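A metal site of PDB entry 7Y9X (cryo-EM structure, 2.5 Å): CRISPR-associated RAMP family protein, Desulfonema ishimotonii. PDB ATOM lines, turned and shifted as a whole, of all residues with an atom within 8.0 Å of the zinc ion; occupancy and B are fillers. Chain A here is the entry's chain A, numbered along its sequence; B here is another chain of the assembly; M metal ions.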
ATOM      1  N   ARG A 452      -1.349 -39.320 -21.142  1.00  0.00           N
ATOM      2  CA  ARG A 452      -0.423 -38.189 -21.057  1.00  0.00           C
ATOM      3  C   ARG A 452       0.775 -38.397 -21.964  1.00  0.00           C
ATOM      4  O   ARG A 452       1.219 -37.459 -22.643  1.00  0.00           O
ATOM      5  CB  ARG A 452       0.029 -37.990 -19.601  1.00  0.00           C
ATOM      6  CG  ARG A 452       0.978 -36.835 -19.412  1.00  0.00           C
ATOM      7  CD  ARG A 452       1.377 -36.664 -17.963  1.00  0.00           C
ATOM      8  NE  ARG A 452       0.240 -36.372 -17.095  1.00  0.00           N
ATOM      9  CZ  ARG A 452      -0.230 -35.155 -16.876  1.00  0.00           C
ATOM     10  NH1 ARG A 452       0.290 -34.090 -17.469  1.00  0.00           N
ATOM     11  NH2 ARG A 452      -1.239 -34.989 -16.024  1.00  0.00           N
ATOM     12  N   GLN A 456       1.483 -36.049 -25.432  1.00  0.00           N
ATOM     13  CA  GLN A 456       2.778 -35.437 -25.710  1.00  0.00           C
ATOM     14  C   GLN A 456       3.371 -35.954 -27.007  1.00  0.00           C
ATOM     15  O   GLN A 456       4.124 -35.232 -27.662  1.00  0.00           O
ATOM     16  CB  GLN A 456       3.740 -35.692 -24.558  1.00  0.00           C
ATOM     17  CG  GLN A 456       3.285 -35.121 -23.234  1.00  0.00           C
ATOM     18  CD  GLN A 456       4.263 -35.412 -22.123  1.00  0.00           C
ATOM     19  OE1 GLN A 456       5.443 -35.128 -22.243  1.00  0.00           O
ATOM     20  NE2 GLN A 456       3.764 -35.993 -21.052  1.00  0.00           N
ATOM     21  N   SER A 461       5.727 -32.536 -28.081  1.00  0.00           N
ATOM     22  CA  SER A 461       6.204 -31.542 -27.122  1.00  0.00           C
ATOM     23  C   SER A 461       6.311 -32.179 -25.746  1.00  0.00           C
ATOM     24  O   SER A 461       5.295 -32.388 -25.072  1.00  0.00           O
ATOM     25  CB  SER A 461       5.280 -30.330 -27.078  1.00  0.00           C
ATOM     26  OG  SER A 461       5.184 -29.704 -28.343  1.00  0.00           O
ATOM     27  N   PRO A 462       7.526 -32.505 -25.300  1.00  0.00           N
ATOM     28  CA  PRO A 462       7.702 -32.961 -23.924  1.00  0.00           C
ATOM     29  C   PRO A 462       7.290 -31.879 -22.934  1.00  0.00           C
ATOM     30  O   PRO A 462       7.464 -30.687 -23.178  1.00  0.00           O
ATOM     31  CB  PRO A 462       9.198 -33.245 -23.831  1.00  0.00           C
ATOM     32  CG  PRO A 462       9.574 -33.576 -25.228  1.00  0.00           C
ATOM     33  CD  PRO A 462       8.778 -32.605 -26.063  1.00  0.00           C
ATOM     34  N   CYS A 463       6.737 -32.312 -21.808  1.00  0.00           N
ATOM     35  CA  CYS A 463       6.430 -31.432 -20.700  1.00  0.00           C
ATOM     36  C   CYS A 463       7.533 -31.563 -19.647  1.00  0.00           C
ATOM     37  O   CYS A 463       7.838 -32.670 -19.210  1.00  0.00           O
ATOM     38  CB  CYS A 463       5.082 -31.768 -20.086  1.00  0.00           C
ATOM     39  SG  CYS A 463       4.591 -30.661 -18.759  1.00  0.00           S
ATOM     40  N   ASN A 464       8.117 -30.430 -19.263  1.00  0.00           N
ATOM     41  CA  ASN A 464       9.179 -30.415 -18.264  1.00  0.00           C
ATOM     42  C   ASN A 464       8.697 -29.863 -16.934  1.00  0.00           C
ATOM     43  O   ASN A 464       9.512 -29.406 -16.120  1.00  0.00           O
ATOM     44  CB  ASN A 464      10.384 -29.603 -18.779  1.00  0.00           C
ATOM     45  CG  ASN A 464      10.056 -28.144 -18.993  1.00  0.00           C
ATOM     46  OD1 ASN A 464       8.902 -27.741 -19.005  1.00  0.00           O
ATOM     47  ND2 ASN A 464      11.094 -27.336 -19.161  1.00  0.00           N
ATOM     48  N   ALA A 465       7.390 -29.898 -16.688  1.00  0.00           N
ATOM     49  CA  ALA A 465       6.861 -29.402 -15.426  1.00  0.00           C
ATOM     50  C   ALA A 465       7.319 -30.264 -14.263  1.00  0.00           C
ATOM     51  O   ALA A 465       7.513 -31.480 -14.388  1.00  0.00           O
ATOM     52  CB  ALA A 465       5.329 -29.352 -15.478  1.00  0.00           C
ATOM     53  N   GLU A 466       7.497 -29.627 -13.115  1.00  0.00           N
ATOM     54  CA  GLU A 466       7.895 -30.289 -11.894  1.00  0.00           C
ATOM     55  C   GLU A 466       6.686 -30.444 -10.983  1.00  0.00           C
ATOM     56  O   GLU A 466       5.684 -29.744 -11.122  1.00  0.00           O
ATOM     57  CB  GLU A 466       8.993 -29.494 -11.182  1.00  0.00           C
ATOM     58  CG  GLU A 466      10.261 -29.324 -12.006  1.00  0.00           C
ATOM     59  CD  GLU A 466      11.040 -30.612 -12.140  1.00  0.00           C
ATOM     60  OE1 GLU A 466      10.902 -31.490 -11.256  1.00  0.00           O
ATOM     61  OE2 GLU A 466      11.773 -30.758 -13.127  1.00  0.00           O
ATOM     62  N   PRO A 471      -0.473 -25.063 -11.844  1.00  0.00           N
ATOM     63  CA  PRO A 471      -0.598 -26.108 -12.863  1.00  0.00           C
ATOM     64  C   PRO A 471       0.033 -25.685 -14.183  1.00  0.00           C
ATOM     65  O   PRO A 471      -0.056 -24.531 -14.607  1.00  0.00           O
ATOM     66  CB  PRO A 471      -2.106 -26.300 -13.000  1.00  0.00           C
ATOM     67  CG  PRO A 471      -2.660 -25.833 -11.722  1.00  0.00           C
ATOM     68  CD  PRO A 471      -1.784 -24.712 -11.270  1.00  0.00           C
ATOM     69  N   CYS A 472       0.672 -26.642 -14.842  1.00  0.00           N
ATOM     70  CA  CYS A 472       1.323 -26.362 -16.110  1.00  0.00           C
ATOM     71  C   CYS A 472       0.287 -26.071 -17.186  1.00  0.00           C
ATOM     72  O   CYS A 472      -0.790 -26.653 -17.217  1.00  0.00           O
ATOM     73  CB  CYS A 472       2.221 -27.528 -16.517  1.00  0.00           C
ATOM     74  SG  CYS A 472       2.822 -27.407 -18.193  1.00  0.00           S
ATOM     75  N   MET A 473       0.647 -25.152 -18.086  1.00  0.00           N
ATOM     76  CA  MET A 473      -0.282 -24.629 -19.085  1.00  0.00           C
ATOM     77  C   MET A 473       0.020 -25.121 -20.489  1.00  0.00           C
ATOM     78  O   MET A 473      -0.437 -24.497 -21.457  1.00  0.00           O
ATOM     79  CB  MET A 473      -0.290 -23.107 -19.043  1.00  0.00           C
ATOM     80  CG  MET A 473      -1.015 -22.535 -17.855  1.00  0.00           C
ATOM     81  SD  MET A 473      -2.748 -23.037 -17.833  1.00  0.00           S
ATOM     82  CE  MET A 473      -3.239 -22.457 -16.229  1.00  0.00           C
ATOM     83  N   CYS A 474       0.768 -26.207 -20.643  1.00  0.00           N
ATOM     84  CA  CYS A 474       0.941 -26.755 -21.972  1.00  0.00           C
ATOM     85  C   CYS A 474      -0.334 -27.459 -22.414  1.00  0.00           C
ATOM     86  O   CYS A 474      -1.249 -27.723 -21.633  1.00  0.00           O
ATOM     87  CB  CYS A 474       2.134 -27.711 -22.035  1.00  0.00           C
ATOM     88  SG  CYS A 474       1.944 -29.317 -21.236  1.00  0.00           S
ATOM     89  N   LYS A 475      -0.387 -27.776 -23.709  1.00  0.00           N
ATOM     90  CA  LYS A 475      -1.574 -28.373 -24.296  1.00  0.00           C
ATOM     91  C   LYS A 475      -1.873 -29.735 -23.692  1.00  0.00           C
ATOM     92  O   LYS A 475      -3.046 -30.092 -23.516  1.00  0.00           O
ATOM     93  CB  LYS A 475      -1.397 -28.470 -25.806  1.00  0.00           C
ATOM     94  CG  LYS A 475      -1.133 -27.138 -26.485  1.00  0.00           C
ATOM     95  CD  LYS A 475      -0.785 -27.329 -27.945  1.00  0.00           C
ATOM     96  CE  LYS A 475      -0.459 -25.999 -28.599  1.00  0.00           C
ATOM     97  NZ  LYS A 475      -0.084 -26.150 -30.033  1.00  0.00           N
ATOM     98  N   THR A 476      -0.844 -30.516 -23.375  1.00  0.00           N
ATOM     99  CA  THR A 476      -1.053 -31.827 -22.779  1.00  0.00           C
ATOM    100  C   THR A 476      -1.651 -31.726 -21.379  1.00  0.00           C
ATOM    101  O   THR A 476      -2.615 -32.432 -21.046  1.00  0.00           O
ATOM    102  CB  THR A 476       0.253 -32.613 -22.738  1.00  0.00           C
ATOM    103  OG1 THR A 476       0.758 -32.778 -24.071  1.00  0.00           O
ATOM    104  CG2 THR A 476       0.038 -33.980 -22.117  1.00  0.00           C
ATOM    105  N   CYS A 477      -1.091 -30.848 -20.541  1.00  0.00           N
ATOM    106  CA  CYS A 477      -1.544 -30.763 -19.159  1.00  0.00           C
ATOM    107  C   CYS A 477      -2.954 -30.195 -19.064  1.00  0.00           C
ATOM    108  O   CYS A 477      -3.696 -30.524 -18.140  1.00  0.00           O
ATOM    109  CB  CYS A 477      -0.574 -29.909 -18.334  1.00  0.00           C
ATOM    110  SG  CYS A 477       0.939 -30.750 -17.834  1.00  0.00           S
ATOM    111  N   ARG A 478      -3.323 -29.302 -19.985  1.00  0.00           N
ATOM    112  CA  ARG A 478      -4.671 -28.743 -19.944  1.00  0.00           C
ATOM    113  C   ARG A 478      -5.709 -29.749 -20.414  1.00  0.00           C
ATOM    114  O   ARG A 478      -6.844 -29.747 -19.928  1.00  0.00           O
ATOM    115  CB  ARG A 478      -4.732 -27.459 -20.779  1.00  0.00           C
ATOM    116  CG  ARG A 478      -3.999 -26.297 -20.127  1.00  0.00           C
ATOM    117  CD  ARG A 478      -4.192 -24.976 -20.841  1.00  0.00           C
ATOM    118  NE  ARG A 478      -3.409 -24.865 -22.057  1.00  0.00           N
ATOM    119  CZ  ARG A 478      -3.909 -24.899 -23.285  1.00  0.00           C
ATOM    120  NH1 ARG A 478      -5.209 -25.020 -23.498  1.00  0.00           N
ATOM    121  NH2 ARG A 478      -3.082 -24.791 -24.327  1.00  0.00           N
ATOM    122  N   ARG A 481      -6.207 -32.321 -17.575  1.00  0.00           N
ATOM    123  CA  ARG A 481      -7.044 -31.823 -16.494  1.00  0.00           C
ATOM    124  C   ARG A 481      -8.524 -31.861 -16.839  1.00  0.00           C
ATOM    125  O   ARG A 481      -9.345 -31.604 -15.953  1.00  0.00           O
ATOM    126  CB  ARG A 481      -6.626 -30.406 -16.106  1.00  0.00           C
ATOM    127  CG  ARG A 481      -5.321 -30.336 -15.342  1.00  0.00           C
ATOM    128  CD  ARG A 481      -5.145 -29.010 -14.621  1.00  0.00           C
ATOM    129  NE  ARG A 481      -4.962 -27.896 -15.545  1.00  0.00           N
ATOM    130  CZ  ARG A 481      -3.798 -27.498 -16.021  1.00  0.00           C
ATOM    131  NH1 ARG A 481      -2.672 -28.122 -15.704  1.00  0.00           N
ATOM    132  NH2 ARG A 481      -3.749 -26.463 -16.842  1.00  0.00           N
ATOM    133  N   MET B 620       9.336 -26.445 -24.645  1.00  0.00           N
ATOM    134  CA  MET B 620       9.623 -25.916 -23.313  1.00  0.00           C
ATOM    135  C   MET B 620      11.011 -26.322 -22.856  1.00  0.00           C
ATOM    136  O   MET B 620      11.716 -25.526 -22.221  1.00  0.00           O
ATOM    137  CB  MET B 620       8.585 -26.407 -22.308  1.00  0.00           C
ATOM    138  CG  MET B 620       7.155 -26.103 -22.665  1.00  0.00           C
ATOM    139  SD  MET B 620       6.020 -26.771 -21.429  1.00  0.00           S
ATOM    140  CE  MET B 620       4.751 -25.510 -21.454  1.00  0.00           C
HETATM  141 ZN    ZN M   1       2.563 -29.556 -19.008  1.00  0.00          ZN
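The nearest printed residue that does not touch the zinc ion is Ala 465 (4.5 Å).
The zinc ion is bound by the side-chain sulfur (SG) of Cys 472 (2.3 Å), the side-chain sulfur (SG) of Cys 463 (2.3 Å), the side-chain sulfur (SG) of Cys 474 (2.3 Å) and the side-chain sulfur (SG) of Cys 477 (2.3 Å). The zinc ion has four donor atoms within binding distance.
The backbone carbonyl oxygen of Cys 472 sits at hydrogen-bond distance from the guanidinium group of Arg 481, at 2.8 Å. SG of Cys 463 sits close to N of Ala 465 (3.6 Å). N of Cys 463 is in hydrogen-bond range of OE1 of Gln 456, 3.1 Å away. The side-chain sulfur (SG) of Cys 474 sits close to the backbone NH (N) of Thr 476. SG of Cys 477 lies close to NH1 of Arg 452.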
